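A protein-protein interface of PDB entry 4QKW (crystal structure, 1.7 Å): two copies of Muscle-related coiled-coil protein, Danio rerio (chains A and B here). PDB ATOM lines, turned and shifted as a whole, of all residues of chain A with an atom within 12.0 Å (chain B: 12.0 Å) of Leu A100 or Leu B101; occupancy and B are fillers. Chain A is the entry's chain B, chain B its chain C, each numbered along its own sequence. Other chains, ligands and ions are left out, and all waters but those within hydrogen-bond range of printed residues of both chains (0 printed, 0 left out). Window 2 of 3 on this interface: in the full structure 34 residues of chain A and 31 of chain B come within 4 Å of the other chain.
Hydrophobic or aromatic side chains of chain B that line the printed part of chain A: Val B93 and Leu B101. Of the 14 printed residues of chain A, 4 touch a printed residue of chain B. Along chain A the printed residues that touch a printed residue of chain B span positions 93 to 100. Among the printed residues, 6 pairs touch across the chains. Among the printed residues, no Asp or Glu carboxylate lies within 4 Å of a Lys or Arg side-chain nitrogen of the other chain.
The side-chain hydroxyl of Thr A96 sits at hydrogen-bond distance from the backbone carbonyl oxygen of Lys A92, at 3.2 Å.
Among the printed residues, merely in contact across the chains: Val A93 with Val B93 (3.4 Å), Thr A96 with Gln B97 (3.5 Å), Gln A97 with Gln B97 (3.6 Å), Val A93 with Glu B94 (3.8 Å) and Leu A100 with Leu B101 (3.95 Å).
Of the printed residues of chain B, Val A93 touches Val B93, Glu B94 and Gln B97. Thr A96 touches one residue of chain B. No residue of chain B comes within 4 Å of Asp A98. No residue of chain B comes within 4 Å of Glu A99. Of chain B, only Leu B101 comes within 4 Å of Leu A100. Leu A101 touches none of the printed residues of chain B. No residue of chain B comes within 4 Å of Thr A102. Printed residues of chain A within 4 Å of Val B93: Val A93. Of the printed residues of chain A, Glu B94 touches Val A93 (3.8 Å). Of chain A, only Val A93 (3.0 Å), Thr A96 (3.5 Å) and Gln A97 (3.6 Å) come within 4 Å of Gln B97. No residue of chain A comes within 4 Å of Asp B98. No residue of chain A comes within 4 Å of Glu B99. No residue of chain A comes within 4 Å of Leu B100. Leu B101 touches one residue of chain A. The nearest residue of chain B that does not touch Leu A100 is Gln B97 (4.8 Å). The nearest residue of chain A that does not touch Leu B101 is Thr A96 (6.7 Å). The nearest printed residue of chain A that does not touch Glu B94 is Lys A92 (5.6 Å).
O of Val A93 sits at hydrogen-bond distance from NE2 of Gln B97 (3.0 Å).
Val A93 touches Glu B94, but with the chains exchanged Glu A94 does not touch Val B93 (6.7 Å). Thr A96 touches Gln B97, but with the chains exchanged Gln A97 does not touch Thr B96 (7.8 Å). Gln B97 touches its own counterpart, Gln A97. Leu A100 touches Leu B101, but with the chains exchanged Leu A101 does not touch Leu B100 (9.0 Å).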
ATOM      1  N   VAL A  90      33.907   8.025  16.028  1.00  0.00           N
ATOM      2  CA  VAL A  90      34.579   9.091  16.771  1.00  0.00           C
ATOM      3  C   VAL A  90      34.231  10.459  16.206  1.00  0.00           C
ATOM      4  O   VAL A  90      33.944  11.394  16.970  1.00  0.00           O
ATOM      5  CB  VAL A  90      36.115   8.884  16.776  1.00  0.00           C
ATOM      6  CG1 VAL A  90      36.807  10.110  17.367  1.00  0.00           C
ATOM      7  CG2 VAL A  90      36.467   7.631  17.553  1.00  0.00           C
ATOM      8  N   LYS A  91      34.218  10.583  14.879  1.00  0.00           N
ATOM      9  CA  LYS A  91      33.868  11.844  14.225  1.00  0.00           C
ATOM     10  C   LYS A  91      32.463  12.264  14.672  1.00  0.00           C
ATOM     11  O   LYS A  91      32.191  13.443  14.970  1.00  0.00           O
ATOM     12  CB  LYS A  91      33.933  11.688  12.704  1.00  0.00           C
ATOM     13  CG  LYS A  91      33.956  12.994  11.920  1.00  0.00           C
ATOM     14  CD  LYS A  91      34.430  12.751  10.489  1.00  0.00           C
ATOM     15  CE  LYS A  91      34.885  14.039   9.819  1.00  0.00           C
ATOM     16  NZ  LYS A  91      35.247  13.816   8.388  1.00  0.00           N
ATOM     17  N   LYS A  92      31.580  11.277  14.739  1.00  0.00           N
ATOM     18  CA  LYS A  92      30.193  11.477  15.133  1.00  0.00           C
ATOM     19  C   LYS A  92      30.101  12.139  16.507  1.00  0.00           C
ATOM     20  O   LYS A  92      29.381  13.131  16.699  1.00  0.00           O
ATOM     21  CB  LYS A  92      29.509  10.114  15.162  1.00  0.00           C
ATOM     22  CG  LYS A  92      28.024  10.130  15.373  1.00  0.00           C
ATOM     23  CD  LYS A  92      27.438   8.837  14.822  1.00  0.00           C
ATOM     24  CE  LYS A  92      25.950   8.728  15.060  1.00  0.00           C
ATOM     25  NZ  LYS A  92      25.374   7.590  14.291  1.00  0.00           N
ATOM     26  N   VAL A  93      30.835  11.589  17.463  1.00  0.00           N
ATOM     27  CA  VAL A  93      30.800  12.111  18.814  1.00  0.00           C
ATOM     28  C   VAL A  93      31.518  13.462  18.897  1.00  0.00           C
ATOM     29  O   VAL A  93      31.039  14.381  19.575  1.00  0.00           O
ATOM     30  CB  VAL A  93      31.420  11.132  19.819  1.00  0.00           C
ATOM     31  CG1 VAL A  93      31.432  11.771  21.180  1.00  0.00           C
ATOM     32  CG2 VAL A  93      30.627   9.841  19.857  1.00  0.00           C
ATOM     33  N   GLU A  94      32.641  13.587  18.190  1.00  0.00           N
ATOM     34  CA  GLU A  94      33.406  14.837  18.138  1.00  0.00           C
ATOM     35  C   GLU A  94      32.574  15.995  17.615  1.00  0.00           C
ATOM     36  O   GLU A  94      32.579  17.082  18.196  1.00  0.00           O
ATOM     37  CB  GLU A  94      34.612  14.715  17.189  1.00  0.00           C
ATOM     38  CG  GLU A  94      35.757  13.841  17.630  1.00  0.00           C
ATOM     39  CD  GLU A  94      36.808  13.691  16.532  1.00  0.00           C
ATOM     40  OE1 GLU A  94      36.433  13.491  15.354  1.00  0.00           O
ATOM     41  OE2 GLU A  94      38.010  13.788  16.846  1.00  0.00           O
ATOM     42  N   THR A  95      31.899  15.776  16.486  1.00  0.00           N
ATOM     43  CA  THR A  95      31.165  16.846  15.826  1.00  0.00           C
ATOM     44  C   THR A  95      30.039  17.317  16.740  1.00  0.00           C
ATOM     45  O   THR A  95      29.780  18.517  16.863  1.00  0.00           O
ATOM     46  CB  THR A  95      30.572  16.389  14.478  1.00  0.00           C
ATOM     47  OG1 THR A  95      31.621  15.886  13.637  1.00  0.00           O
ATOM     48  CG2 THR A  95      29.885  17.550  13.778  1.00  0.00           C
ATOM     49  N   THR A  96      29.388  16.369  17.405  1.00  0.00           N
ATOM     50  CA  THR A  96      28.277  16.705  18.303  1.00  0.00           C
ATOM     51  C   THR A  96      28.755  17.447  19.556  1.00  0.00           C
ATOM     52  O   THR A  96      28.103  18.380  20.030  1.00  0.00           O
ATOM     53  CB  THR A  96      27.490  15.445  18.682  1.00  0.00           C
ATOM     54  OG1 THR A  96      26.866  14.924  17.499  1.00  0.00           O
ATOM     55  CG2 THR A  96      26.407  15.769  19.714  1.00  0.00           C
ATOM     56  N   GLN A  97      29.894  17.035  20.095  1.00  0.00           N
ATOM     57  CA  GLN A  97      30.440  17.720  21.265  1.00  0.00           C
ATOM     58  C   GLN A  97      30.777  19.165  20.900  1.00  0.00           C
ATOM     59  O   GLN A  97      30.498  20.110  21.659  1.00  0.00           O
ATOM     60  CB  GLN A  97      31.669  16.969  21.765  1.00  0.00           C
ATOM     61  CG  GLN A  97      32.161  17.375  23.133  1.00  0.00           C
ATOM     62  CD  GLN A  97      33.243  16.432  23.616  1.00  0.00           C
ATOM     63  OE1 GLN A  97      34.384  16.497  23.158  1.00  0.00           O
ATOM     64  NE2 GLN A  97      32.880  15.528  24.522  1.00  0.00           N
ATOM     65  N   ASP A  98      31.343  19.352  19.713  1.00  0.00           N
ATOM     66  CA  ASP A  98      31.655  20.699  19.253  1.00  0.00           C
ATOM     67  C   ASP A  98      30.379  21.530  19.094  1.00  0.00           C
ATOM     68  O   ASP A  98      30.338  22.708  19.463  1.00  0.00           O
ATOM     69  CB  ASP A  98      32.445  20.656  17.943  1.00  0.00           C
ATOM     70  CG  ASP A  98      33.840  20.094  18.120  1.00  0.00           C
ATOM     71  OD1 ASP A  98      34.401  20.213  19.234  1.00  0.00           O
ATOM     72  OD2 ASP A  98      34.379  19.544  17.136  1.00  0.00           O
ATOM     73  N   GLU A  99      29.331  20.902  18.565  1.00  0.00           N
ATOM     74  CA  GLU A  99      28.021  21.530  18.442  1.00  0.00           C
ATOM     75  C   GLU A  99      27.509  21.997  19.809  1.00  0.00           C
ATOM     76  O   GLU A  99      27.004  23.116  19.964  1.00  0.00           O
ATOM     77  CB  GLU A  99      27.037  20.524  17.838  1.00  0.00           C
ATOM     78  CG  GLU A  99      25.578  20.952  17.903  1.00  0.00           C
ATOM     79  CD  GLU A  99      25.137  21.694  16.662  1.00  0.00           C
ATOM     80  OE1 GLU A  99      25.930  21.757  15.700  1.00  0.00           O
ATOM     81  OE2 GLU A  99      23.996  22.206  16.640  1.00  0.00           O
ATOM     82  N   LEU A 100      27.655  21.134  20.809  1.00  0.00           N
ATOM     83  CA  LEU A 100      27.151  21.431  22.147  1.00  0.00           C
ATOM     84  C   LEU A 100      27.923  22.581  22.795  1.00  0.00           C
ATOM     85  O   LEU A 100      27.375  23.329  23.597  1.00  0.00           O
ATOM     86  CB  LEU A 100      27.225  20.185  23.032  1.00  0.00           C
ATOM     87  CG  LEU A 100      26.327  19.005  22.657  1.00  0.00           C
ATOM     88  CD1 LEU A 100      26.659  17.790  23.519  1.00  0.00           C
ATOM     89  CD2 LEU A 100      24.865  19.392  22.805  1.00  0.00           C
ATOM     90  N   LEU A 101      29.195  22.725  22.441  1.00  0.00           N
ATOM     91  CA  LEU A 101      30.051  23.760  23.027  1.00  0.00           C
ATOM     92  C   LEU A 101      29.920  25.082  22.287  1.00  0.00           C
ATOM     93  O   LEU A 101      30.539  26.088  22.651  1.00  0.00           O
ATOM     94  CB  LEU A 101      31.512  23.290  23.057  1.00  0.00           C
ATOM     95  CG  LEU A 101      31.732  22.124  24.013  1.00  0.00           C
ATOM     96  CD1 LEU A 101      33.134  21.536  23.845  1.00  0.00           C
ATOM     97  CD2 LEU A 101      31.516  22.587  25.438  1.00  0.00           C
ATOM     98  N   THR A 102      29.078  25.088  21.262  1.00  0.00           N
ATOM     99  CA  THR A 102      28.770  26.314  20.525  1.00  0.00           C
ATOM    100  C   THR A 102      27.722  27.191  21.234  1.00  0.00           C
ATOM    101  O   THR A 102      26.858  26.680  21.960  1.00  0.00           O
ATOM    102  CB  THR A 102      28.301  25.979  19.088  1.00  0.00           C
ATOM    103  OG1 THR A 102      29.323  25.220  18.422  1.00  0.00           O
ATOM    104  CG2 THR A 102      28.002  27.234  18.282  1.00  0.00           C
ATOM    105  N   ARG A 103      27.861  28.506  21.037  1.00  0.00           N
ATOM    106  CA  ARG A 103      26.871  29.562  21.350  1.00  0.00           C
ATOM    107  C   ARG A 103      27.243  30.504  22.488  1.00  0.00           C
ATOM    108  O   ARG A 103      27.146  31.720  22.326  1.00  0.00           O
ATOM    109  CB  ARG A 103      25.421  29.061  21.491  1.00  0.00           C
ATOM    110  CG  ARG A 103      24.828  28.620  20.170  1.00  0.00           C
ATOM    111  CD  ARG A 103      24.925  29.744  19.154  1.00  0.00           C
ATOM    112  NE  ARG A 103      25.143  29.263  17.793  1.00  0.00           N
ATOM    113  CZ  ARG A 103      25.588  30.027  16.801  1.00  0.00           C
ATOM    114  NH1 ARG A 103      25.865  31.305  17.025  1.00  0.00           N
ATOM    115  NH2 ARG A 103      25.763  29.519  15.589  1.00  0.00           N
ATOM    116  N   LYS B  92      31.535   3.869  25.440  1.00  0.00           N
ATOM    117  CA  LYS B  92      31.224   4.599  26.670  1.00  0.00           C
ATOM    118  C   LYS B  92      30.938   6.070  26.379  1.00  0.00           C
ATOM    119  O   LYS B  92      30.003   6.671  26.929  1.00  0.00           O
ATOM    120  CB  LYS B  92      32.367   4.474  27.684  1.00  0.00           C
ATOM    121  CG  LYS B  92      32.144   5.302  28.942  1.00  0.00           C
ATOM    122  CD  LYS B  92      33.180   5.009  30.010  1.00  0.00           C
ATOM    123  CE  LYS B  92      32.937   5.862  31.249  1.00  0.00           C
ATOM    124  NZ  LYS B  92      34.177   6.030  32.062  1.00  0.00           N
ATOM    125  N   VAL B  93      31.755   6.648  25.512  1.00  0.00           N
ATOM    126  CA  VAL B  93      31.586   8.031  25.115  1.00  0.00           C
ATOM    127  C   VAL B  93      30.271   8.259  24.351  1.00  0.00           C
ATOM    128  O   VAL B  93      29.572   9.255  24.585  1.00  0.00           O
ATOM    129  CB  VAL B  93      32.774   8.485  24.283  1.00  0.00           C
ATOM    130  CG1 VAL B  93      32.491   9.800  23.697  1.00  0.00           C
ATOM    131  CG2 VAL B  93      34.019   8.559  25.158  1.00  0.00           C
ATOM    132  N   GLU B  94      29.939   7.333  23.452  1.00  0.00           N
ATOM    133  CA  GLU B  94      28.678   7.369  22.715  1.00  0.00           C
ATOM    134  C   GLU B  94      27.485   7.318  23.662  1.00  0.00           C
ATOM    135  O   GLU B  94      26.548   8.110  23.534  1.00  0.00           O
ATOM    136  CB  GLU B  94      28.603   6.189  21.740  1.00  0.00           C
ATOM    137  CG  GLU B  94      29.555   6.311  20.563  1.00  0.00           C
ATOM    138  CD  GLU B  94      29.604   5.048  19.726  1.00  0.00           C
ATOM    139  OE1 GLU B  94      29.588   3.934  20.305  1.00  0.00           O
ATOM    140  OE2 GLU B  94      29.656   5.172  18.484  1.00  0.00           O
ATOM    141  N   THR B  95      27.530   6.375  24.600  1.00  0.00           N
ATOM    142  CA  THR B  95      26.462   6.176  25.574  1.00  0.00           C
ATOM    143  C   THR B  95      26.283   7.414  26.449  1.00  0.00           C
ATOM    144  O   THR B  95      25.160   7.838  26.726  1.00  0.00           O
ATOM    145  CB  THR B  95      26.765   4.961  26.483  1.00  0.00           C
ATOM    146  OG1 THR B  95      26.927   3.783  25.679  1.00  0.00           O
ATOM    147  CG2 THR B  95      25.639   4.740  27.479  1.00  0.00           C
ATOM    148  N   THR B  96      27.400   7.995  26.875  1.00  0.00           N
ATOM    149  CA  THR B  96      27.364   9.172  27.737  1.00  0.00           C
ATOM    150  C   THR B  96      26.798  10.389  27.011  1.00  0.00           C
ATOM    151  O   THR B  96      26.021  11.162  27.581  1.00  0.00           O
ATOM    152  CB  THR B  96      28.764   9.501  28.280  1.00  0.00           C
ATOM    153  OG1 THR B  96      29.231   8.402  29.074  1.00  0.00           O
ATOM    154  CG2 THR B  96      28.722  10.769  29.133  1.00  0.00           C
ATOM    155  N   GLN B  97      27.191  10.562  25.753  1.00  0.00           N
ATOM    156  CA  GLN B  97      26.692  11.673  24.955  1.00  0.00           C
ATOM    157  C   GLN B  97      25.190  11.549  24.683  1.00  0.00           C
ATOM    158  O   GLN B  97      24.446  12.527  24.795  1.00  0.00           O
ATOM    159  CB  GLN B  97      27.466  11.775  23.646  1.00  0.00           C
ATOM    160  CG  GLN B  97      27.040  12.962  22.804  1.00  0.00           C
ATOM    161  CD  GLN B  97      27.889  13.128  21.566  1.00  0.00           C
ATOM    162  OE1 GLN B  97      27.636  12.498  20.540  1.00  0.00           O
ATOM    163  NE2 GLN B  97      28.904  13.981  21.656  1.00  0.00           N
ATOM    164  N   ASP B  98      24.750  10.343  24.327  1.00  0.00           N
ATOM    165  CA  ASP B  98      23.327  10.061  24.158  1.00  0.00           C
ATOM    166  C   ASP B  98      22.562  10.406  25.431  1.00  0.00           C
ATOM    167  O   ASP B  98      21.385  10.778  25.378  1.00  0.00           O
ATOM    168  CB  ASP B  98      23.115   8.587  23.813  1.00  0.00           C
ATOM    169  CG  ASP B  98      21.650   8.190  23.815  1.00  0.00           C
ATOM    170  OD1 ASP B  98      20.827   8.911  23.208  1.00  0.00           O
ATOM    171  OD2 ASP B  98      21.321   7.160  24.441  1.00  0.00           O
ATOM    172  N   GLU B  99      23.239  10.287  26.574  1.00  0.00           N
ATOM    173  CA  GLU B  99      22.624  10.554  27.875  1.00  0.00           C
ATOM    174  C   GLU B  99      22.729  12.021  28.304  1.00  0.00           C
ATOM    175  O   GLU B  99      21.766  12.581  28.832  1.00  0.00           O
ATOM    176  CB  GLU B  99      23.215   9.638  28.953  1.00  0.00           C
ATOM    177  CG  GLU B  99      22.173   8.991  29.864  1.00  0.00           C
ATOM    178  CD  GLU B  99      21.472   9.988  30.774  1.00  0.00           C
ATOM    179  OE1 GLU B  99      22.068  11.045  31.073  1.00  0.00           O
ATOM    180  OE2 GLU B  99      20.326   9.712  31.194  1.00  0.00           O
ATOM    181  N   LEU B 100      23.890  12.641  28.078  1.00  0.00           N
ATOM    182  CA  LEU B 100      24.072  14.079  28.310  1.00  0.00           C
ATOM    183  C   LEU B 100      22.983  14.891  27.606  1.00  0.00           C
ATOM    184  O   LEU B 100      22.728  16.039  27.986  1.00  0.00           O
ATOM    185  CB  LEU B 100      25.453  14.541  27.829  1.00  0.00           C
ATOM    186  CG  LEU B 100      26.683  14.296  28.705  1.00  0.00           C
ATOM    187  CD1 LEU B 100      27.949  14.792  28.023  1.00  0.00           C
ATOM    188  CD2 LEU B 100      26.516  14.975  30.048  1.00  0.00           C
ATOM    189  N   LEU B 101      22.397  14.259  26.579  1.00  0.00           N
ATOM    190  CA  LEU B 101      21.225  14.667  25.775  1.00  0.00           C
ATOM    191  C   LEU B 101      21.573  14.661  24.284  1.00  0.00           C
ATOM    192  O   LEU B 101      20.809  14.170  23.456  1.00  0.00           O
ATOM    193  CB  LEU B 101      20.571  15.997  26.207  1.00  0.00           C
ATOM    194  CG  LEU B 101      20.890  17.354  25.553  1.00  0.00           C
ATOM    195  CD1 LEU B 101      20.329  18.488  26.398  1.00  0.00           C
ATOM    196  CD2 LEU B 101      22.379  17.593  25.296  1.00  0.00           C
